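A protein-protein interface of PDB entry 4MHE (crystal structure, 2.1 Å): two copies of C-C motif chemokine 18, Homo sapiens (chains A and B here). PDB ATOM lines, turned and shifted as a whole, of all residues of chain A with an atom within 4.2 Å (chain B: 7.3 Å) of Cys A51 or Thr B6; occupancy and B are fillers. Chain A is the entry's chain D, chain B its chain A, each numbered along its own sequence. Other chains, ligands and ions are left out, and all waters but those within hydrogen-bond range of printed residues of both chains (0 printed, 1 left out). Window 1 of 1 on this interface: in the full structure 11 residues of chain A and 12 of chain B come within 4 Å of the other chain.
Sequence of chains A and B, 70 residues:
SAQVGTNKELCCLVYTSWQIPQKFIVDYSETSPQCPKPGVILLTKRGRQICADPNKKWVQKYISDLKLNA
N of Val B4 is in hydrogen-bond range of O of Gln A49 (2.8 Å). The side-chain amide oxygen (OE1) of Gln A49 lies within hydrogen-bond range of the side-chain amide nitrogen (NE2) of Gln B3, 3.2 Å away. The backbone carbonyl oxygen of Gly B5 lies within hydrogen-bond range of the backbone NH of Val A14. The backbone carbonyl oxygen (O) of Cys A11 is in hydrogen-bond range of the backbone NH (N) of Asn B7 (2.8 Å). The backbone carbonyl oxygen (O) of Val B4 lies within hydrogen-bond range of the backbone NH (N) of Cys A51, 3.0 Å away. The backbone carbonyl oxygen (O) of Ala B2 sits at hydrogen-bond distance from the backbone NH (N) of Gln A49 (2.8 Å).
The side-chain hydroxyl (OG1) of Thr B6 is in hydrogen-bond range of the backbone NH (N) of Glu B9 (3.3 Å). The backbone NH (N) of Ser B32 is in hydrogen-bond range of the backbone carbonyl oxygen (O) of Leu B10, 3.1 Å away. The backbone NH (N) of Thr A16 is in hydrogen-bond range of the backbone carbonyl oxygen (O) of Cys A51. SG of Cys B11 forms a disulfide with SG of Cys B35 (2.0 Å). The side-chain hydroxyl (OG) of Ser B1 sits at hydrogen-bond distance from the backbone carbonyl oxygen (O) of Gln B3 (3.0 Å). The backbone NH (N) of Lys B8 sits close to the side-chain hydroxyl (OG1) of Thr B6, at 3.5 Å.
Leu A10 touches Gln B3 (CD1 to OE1, 3.6 Å). Thr B6 touches Leu A10. CD1 of Leu A10 touches OD1 of Asn B7, at 3.6 Å. CD of Lys B8 touches CD1 of Leu A10, 3.6 Å away. Thr B6 touches Cys A11. Cys A12 touches Gly B5. Leu B10 touches Val A14 (CD1 to CG2, 3.7 Å). CA of Ile A50 touches O of Val B4, at 3.8 Å. Gly B5 touches Cys A51. CG2 of Thr B6 touches SG of Cys A51, 3.4 Å away.
Of the printed residues of chain B, Cys A51 touches Val B4, Gly B5 and Thr B6. Of the printed residues of chain A, Gln B3 touches Leu A10 and Gln A49. Thr B6 touches just these residues of chain A: Leu A10, Cys A11 and Cys A51. Printed residues of chain A within 4 Å of Asn B7: Leu A10 and Cys A11. Glu B9 touches none of the printed residues of chain A. Ser B32 touches none of the printed residues of chain A. The nearest printed residue of chain A that does not touch Thr B6 is Cys A12 (4.3 Å).
Of the 13 printed residues of chain B, 8 touch a printed residue of chain A. Along chain B the printed residues that touch a printed residue of chain A span positions 2 to 10. Among the printed residues, 16 pairs touch across the chains. Among the printed residues, no Asp or Glu carboxylate lies within 4 Å of a Lys or Arg side-chain nitrogen of the other chain.
2 positions are printed for both chains. Of the 16 pairs that touch across the chains among the printed residues, none has its exchanged pair printed and touching as well.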
ATOM      1  N   LEU A  10      11.595  -4.138 -12.308  1.00  0.00           N
ATOM      2  CA  LEU A  10      10.454  -4.270 -11.394  1.00  0.00           C
ATOM      3  C   LEU A  10      10.820  -3.997  -9.921  1.00  0.00           C
ATOM      4  O   LEU A  10      11.712  -4.641  -9.360  1.00  0.00           O
ATOM      5  CB  LEU A  10       9.815  -5.651 -11.523  1.00  0.00           C
ATOM      6  CG  LEU A  10       8.488  -5.803 -10.779  1.00  0.00           C
ATOM      7  CD1 LEU A  10       7.473  -4.801 -11.314  1.00  0.00           C
ATOM      8  CD2 LEU A  10       7.966  -7.211 -10.945  1.00  0.00           C
ATOM      9  N   CYS A  11      10.113  -3.048  -9.304  1.00  0.00           N
ATOM     10  CA  CYS A  11      10.419  -2.598  -7.943  1.00  0.00           C
ATOM     11  C   CYS A  11       9.176  -2.277  -7.112  1.00  0.00           C
ATOM     12  O   CYS A  11       8.119  -1.949  -7.657  1.00  0.00           O
ATOM     13  CB  CYS A  11      11.292  -1.336  -8.000  1.00  0.00           C
ATOM     14  SG  CYS A  11      12.891  -1.590  -8.835  1.00  0.00           S
ATOM     15  N   CYS A  12       9.334  -2.319  -5.787  1.00  0.00           N
ATOM     16  CA  CYS A  12       8.267  -1.951  -4.876  1.00  0.00           C
ATOM     17  C   CYS A  12       8.427  -0.510  -4.424  1.00  0.00           C
ATOM     18  O   CYS A  12       9.537  -0.067  -4.128  1.00  0.00           O
ATOM     19  CB  CYS A  12       8.253  -2.888  -3.673  1.00  0.00           C
ATOM     20  SG  CYS A  12       7.913  -4.598  -4.162  1.00  0.00           S
ATOM     21  N   VAL A  14       5.278   0.964  -2.669  1.00  0.00           N
ATOM     22  CA  VAL A  14       4.379   0.923  -1.524  1.00  0.00           C
ATOM     23  C   VAL A  14       4.190  -0.515  -1.050  1.00  0.00           C
ATOM     24  O   VAL A  14       3.797  -1.389  -1.834  1.00  0.00           O
ATOM     25  CB  VAL A  14       3.002   1.529  -1.878  1.00  0.00           C
ATOM     26  CG1 VAL A  14       2.031   1.394  -0.705  1.00  0.00           C
ATOM     27  CG2 VAL A  14       3.156   2.991  -2.270  1.00  0.00           C
ATOM     28  N   TYR A  15       4.463  -0.750   0.234  1.00  0.00           N
ATOM     29  CA  TYR A  15       4.328  -2.082   0.832  1.00  0.00           C
ATOM     30  C   TYR A  15       2.912  -2.302   1.369  1.00  0.00           C
ATOM     31  O   TYR A  15       2.273  -1.365   1.837  1.00  0.00           O
ATOM     32  CB  TYR A  15       5.305  -2.240   1.990  1.00  0.00           C
ATOM     33  CG  TYR A  15       6.763  -2.047   1.644  1.00  0.00           C
ATOM     34  CD1 TYR A  15       7.334  -2.700   0.571  1.00  0.00           C
ATOM     35  CD2 TYR A  15       7.566  -1.211   2.411  1.00  0.00           C
ATOM     36  CE1 TYR A  15       8.681  -2.528   0.264  1.00  0.00           C
ATOM     37  CE2 TYR A  15       8.892  -1.029   2.121  1.00  0.00           C
ATOM     38  CZ  TYR A  15       9.451  -1.691   1.051  1.00  0.00           C
ATOM     39  OH  TYR A  15      10.784  -1.507   0.774  1.00  0.00           O
ATOM     40  N   THR A  16       2.425  -3.541   1.329  1.00  0.00           N
ATOM     41  CA  THR A  16       1.076  -3.814   1.824  1.00  0.00           C
ATOM     42  C   THR A  16       1.009  -3.816   3.358  1.00  0.00           C
ATOM     43  O   THR A  16       1.904  -4.359   4.033  1.00  0.00           O
ATOM     44  CB  THR A  16       0.516  -5.167   1.300  1.00  0.00           C
ATOM     45  OG1 THR A  16      -0.838  -5.308   1.725  1.00  0.00           O
ATOM     46  CG2 THR A  16       1.294  -6.357   1.877  1.00  0.00           C
ATOM     47  N   VAL A  40       9.773  -7.748  -1.659  1.00  0.00           N
ATOM     48  CA  VAL A  40       9.402  -9.073  -2.124  1.00  0.00           C
ATOM     49  C   VAL A  40       8.019  -8.907  -2.701  1.00  0.00           C
ATOM     50  O   VAL A  40       7.256  -8.044  -2.250  1.00  0.00           O
ATOM     51  CB  VAL A  40       9.350 -10.107  -0.998  1.00  0.00           C
ATOM     52  CG1 VAL A  40      10.501  -9.889  -0.018  1.00  0.00           C
ATOM     53  CG2 VAL A  40       8.040 -10.000  -0.283  1.00  0.00           C
ATOM     54  N   ILE A  41       7.708  -9.707  -3.714  1.00  0.00           N
ATOM     55  CA  ILE A  41       6.385  -9.696  -4.318  1.00  0.00           C
ATOM     56  C   ILE A  41       5.700 -11.013  -3.954  1.00  0.00           C
ATOM     57  O   ILE A  41       6.246 -12.088  -4.196  1.00  0.00           O
ATOM     58  CB  ILE A  41       6.488  -9.504  -5.836  1.00  0.00           C
ATOM     59  CG1 ILE A  41       7.031  -8.094  -6.111  1.00  0.00           C
ATOM     60  CG2 ILE A  41       5.133  -9.748  -6.523  1.00  0.00           C
ATOM     61  CD1 ILE A  41       7.380  -7.832  -7.547  1.00  0.00           C
ATOM     62  N   GLN A  49      -0.118  -9.657  -7.652  1.00  0.00           N
ATOM     63  CA  GLN A  49       1.276  -9.538  -7.250  1.00  0.00           C
ATOM     64  C   GLN A  49       1.395  -8.342  -6.313  1.00  0.00           C
ATOM     65  O   GLN A  49       1.272  -7.186  -6.747  1.00  0.00           O
ATOM     66  CB  GLN A  49       2.163  -9.340  -8.475  1.00  0.00           C
ATOM     67  CG  GLN A  49       2.068 -10.442  -9.522  1.00  0.00           C
ATOM     68  CD  GLN A  49       2.764 -10.046 -10.809  1.00  0.00           C
ATOM     69  OE1 GLN A  49       3.935  -9.653 -10.796  1.00  0.00           O
ATOM     70  NE2 GLN A  49       2.038 -10.113 -11.925  1.00  0.00           N
ATOM     71  N   ILE A  50       1.605  -8.623  -5.028  1.00  0.00           N
ATOM     72  CA  ILE A  50       1.514  -7.599  -3.991  1.00  0.00           C
ATOM     73  C   ILE A  50       2.879  -7.382  -3.338  1.00  0.00           C
ATOM     74  O   ILE A  50       3.479  -8.320  -2.803  1.00  0.00           O
ATOM     75  CB  ILE A  50       0.481  -7.993  -2.921  1.00  0.00           C
ATOM     76  CG1 ILE A  50      -0.884  -8.228  -3.564  1.00  0.00           C
ATOM     77  CG2 ILE A  50       0.339  -6.898  -1.873  1.00  0.00           C
ATOM     78  CD1 ILE A  50      -1.943  -8.617  -2.554  1.00  0.00           C
ATOM     79  N   CYS A  51       3.381  -6.152  -3.411  1.00  0.00           N
ATOM     80  CA  CYS A  51       4.659  -5.809  -2.788  1.00  0.00           C
ATOM     81  C   CYS A  51       4.506  -5.828  -1.280  1.00  0.00           C
ATOM     82  O   CYS A  51       3.480  -5.408  -0.744  1.00  0.00           O
ATOM     83  CB  CYS A  51       5.113  -4.411  -3.213  1.00  0.00           C
ATOM     84  SG  CYS A  51       5.974  -4.314  -4.817  1.00  0.00           S
ATOM     85  N   ALA A  52       5.538  -6.317  -0.600  1.00  0.00           N
ATOM     86  CA  ALA A  52       5.547  -6.401   0.846  1.00  0.00           C
ATOM     87  C   ALA A  52       6.957  -6.117   1.325  1.00  0.00           C
ATOM     88  O   ALA A  52       7.924  -6.308   0.576  1.00  0.00           O
ATOM     89  CB  ALA A  52       5.092  -7.800   1.304  1.00  0.00           C
ATOM     90  N   SER B   1      -4.619  -4.419 -13.499  1.00  0.00           N
ATOM     91  CA  SER B   1      -3.640  -4.151 -12.461  1.00  0.00           C
ATOM     92  C   SER B   1      -3.411  -5.389 -11.593  1.00  0.00           C
ATOM     93  O   SER B   1      -3.821  -5.440 -10.427  1.00  0.00           O
ATOM     94  CB  SER B   1      -4.097  -2.978 -11.602  1.00  0.00           C
ATOM     95  OG  SER B   1      -3.074  -2.581 -10.705  1.00  0.00           O
ATOM     96  N   ALA B   2      -2.751  -6.391 -12.166  1.00  0.00           N
ATOM     97  CA  ALA B   2      -2.359  -7.565 -11.407  1.00  0.00           C
ATOM     98  C   ALA B   2      -1.463  -7.133 -10.249  1.00  0.00           C
ATOM     99  O   ALA B   2      -1.409  -7.782  -9.201  1.00  0.00           O
ATOM    100  CB  ALA B   2      -1.628  -8.526 -12.298  1.00  0.00           C
ATOM    101  N   GLN B   3      -0.774  -6.016 -10.447  1.00  0.00           N
ATOM    102  CA  GLN B   3       0.260  -5.582  -9.522  1.00  0.00           C
ATOM    103  C   GLN B   3      -0.170  -4.482  -8.564  1.00  0.00           C
ATOM    104  O   GLN B   3      -0.854  -3.521  -8.947  1.00  0.00           O
ATOM    105  CB  GLN B   3       1.501  -5.137 -10.296  1.00  0.00           C
ATOM    106  CG  GLN B   3       2.296  -6.280 -10.880  1.00  0.00           C
ATOM    107  CD  GLN B   3       3.556  -5.798 -11.551  1.00  0.00           C
ATOM    108  OE1 GLN B   3       3.839  -4.591 -11.577  1.00  0.00           O
ATOM    109  NE2 GLN B   3       4.323  -6.732 -12.108  1.00  0.00           N
ATOM    110  N   VAL B   4       0.295  -4.619  -7.326  1.00  0.00           N
ATOM    111  CA  VAL B   4      -0.017  -3.699  -6.247  1.00  0.00           C
ATOM    112  C   VAL B   4       1.261  -3.179  -5.594  1.00  0.00           C
ATOM    113  O   VAL B   4       2.005  -3.964  -4.993  1.00  0.00           O
ATOM    114  CB  VAL B   4      -0.807  -4.420  -5.138  1.00  0.00           C
ATOM    115  CG1 VAL B   4      -0.968  -3.502  -3.924  1.00  0.00           C
ATOM    116  CG2 VAL B   4      -2.170  -4.885  -5.657  1.00  0.00           C
ATOM    117  N   GLY B   5       1.507  -1.868  -5.697  1.00  0.00           N
ATOM    118  CA  GLY B   5       2.614  -1.232  -4.995  1.00  0.00           C
ATOM    119  C   GLY B   5       3.923  -1.152  -5.762  1.00  0.00           C
ATOM    120  O   GLY B   5       4.921  -0.648  -5.245  1.00  0.00           O
ATOM    121  N   THR B   6       3.920  -1.624  -7.006  1.00  0.00           N
ATOM    122  CA  THR B   6       5.135  -1.653  -7.821  1.00  0.00           C
ATOM    123  C   THR B   6       5.291  -0.381  -8.640  1.00  0.00           C
ATOM    124  O   THR B   6       4.335   0.381  -8.818  1.00  0.00           O
ATOM    125  CB  THR B   6       5.120  -2.845  -8.809  1.00  0.00           C
ATOM    126  OG1 THR B   6       4.090  -2.631  -9.786  1.00  0.00           O
ATOM    127  CG2 THR B   6       4.858  -4.155  -8.068  1.00  0.00           C
ATOM    128  N   ASN B   7       6.490  -0.170  -9.169  1.00  0.00           N
ATOM    129  CA  ASN B   7       6.701   0.960 -10.060  1.00  0.00           C
ATOM    130  C   ASN B   7       5.816   0.865 -11.299  1.00  0.00           C
ATOM    131  O   ASN B   7       5.261   1.872 -11.764  1.00  0.00           O
ATOM    132  CB  ASN B   7       8.177   1.061 -10.470  1.00  0.00           C
ATOM    133  CG  ASN B   7       8.730  -0.250 -11.046  1.00  0.00           C
ATOM    134  OD1 ASN B   7       8.078  -1.304 -11.002  1.00  0.00           O
ATOM    135  ND2 ASN B   7       9.950  -0.185 -11.573  1.00  0.00           N
ATOM    136  N   LYS B   8       5.675  -0.342 -11.832  1.00  0.00           N
ATOM    137  CA  LYS B   8       4.943  -0.509 -13.088  1.00  0.00           C
ATOM    138  C   LYS B   8       3.473  -0.123 -12.936  1.00  0.00           C
ATOM    139  O   LYS B   8       2.817   0.234 -13.910  1.00  0.00           O
ATOM    140  CB  LYS B   8       5.117  -1.932 -13.645  1.00  0.00           C
ATOM    141  CG  LYS B   8       6.576  -2.260 -13.977  1.00  0.00           C
ATOM    142  CD  LYS B   8       6.764  -3.629 -14.630  1.00  0.00           C
ATOM    143  CE  LYS B   8       8.243  -3.854 -14.971  1.00  0.00           C
ATOM    144  NZ  LYS B   8       8.557  -5.258 -15.383  1.00  0.00           N
ATOM    145  N   GLU B   9       2.966  -0.173 -11.709  1.00  0.00           N
ATOM    146  CA  GLU B   9       1.591   0.242 -11.442  1.00  0.00           C
ATOM    147  C   GLU B   9       1.459   1.713 -10.990  1.00  0.00           C
ATOM    148  O   GLU B   9       0.418   2.331 -11.177  1.00  0.00           O
ATOM    149  CB  GLU B   9       0.953  -0.679 -10.397  1.00  0.00           C
ATOM    150  CG  GLU B   9       0.748  -0.021  -9.043  1.00  0.00           C
ATOM    151  CD  GLU B   9      -0.714   0.003  -8.618  1.00  0.00           C
ATOM    152  OE1 GLU B   9      -1.585   0.114  -9.517  1.00  0.00           O
ATOM    153  OE2 GLU B   9      -0.985  -0.083  -7.387  1.00  0.00           O
ATOM    154  N   LEU B  10       2.509   2.274 -10.400  1.00  0.00           N
ATOM    155  CA  LEU B  10       2.391   3.601  -9.800  1.00  0.00           C
ATOM    156  C   LEU B  10       3.178   4.682 -10.544  1.00  0.00           C
ATOM    157  O   LEU B  10       3.126   5.862 -10.179  1.00  0.00           O
ATOM    158  CB  LEU B  10       2.807   3.557  -8.321  1.00  0.00           C
ATOM    159  CG  LEU B  10       1.888   2.818  -7.333  1.00  0.00           C
ATOM    160  CD1 LEU B  10       2.536   2.746  -5.952  1.00  0.00           C
ATOM    161  CD2 LEU B  10       0.555   3.539  -7.216  1.00  0.00           C
ATOM    162  N   CYS B  11       3.896   4.278 -11.588  1.00  0.00           N
ATOM    163  CA  CYS B  11       4.758   5.192 -12.322  1.00  0.00           C
ATOM    164  C   CYS B  11       4.449   5.145 -13.803  1.00  0.00           C
ATOM    165  O   CYS B  11       3.918   4.155 -14.312  1.00  0.00           O
ATOM    166  CB  CYS B  11       6.241   4.823 -12.127  1.00  0.00           C
ATOM    167  SG  CYS B  11       6.778   4.805 -10.429  1.00  0.00           S
ATOM    168  N   SER B  32       3.505   8.261  -8.311  1.00  0.00           N
ATOM    169  CA  SER B  32       4.266   8.355  -7.064  1.00  0.00           C
ATOM    170  C   SER B  32       5.440   9.336  -7.155  1.00  0.00           C
ATOM    171  O   SER B  32       6.091   9.456  -8.200  1.00  0.00           O
ATOM    172  CB  SER B  32       4.803   6.985  -6.651  1.00  0.00           C
ATOM    173  OG  SER B  32       5.725   7.143  -5.582  1.00  0.00           O
ATOM    174  N   CYS B  35       8.793   7.964  -8.306  1.00  0.00           N
ATOM    175  CA  CYS B  35       9.078   7.580  -9.692  1.00  0.00           C
ATOM    176  C   CYS B  35      10.284   8.341 -10.234  1.00  0.00           C
ATOM    177  O   CYS B  35      10.420   9.547 -10.023  1.00  0.00           O
ATOM    178  CB  CYS B  35       7.846   7.778 -10.587  1.00  0.00           C
ATOM    179  SG  CYS B  35       6.421   6.766 -10.037  1.00  0.00           S
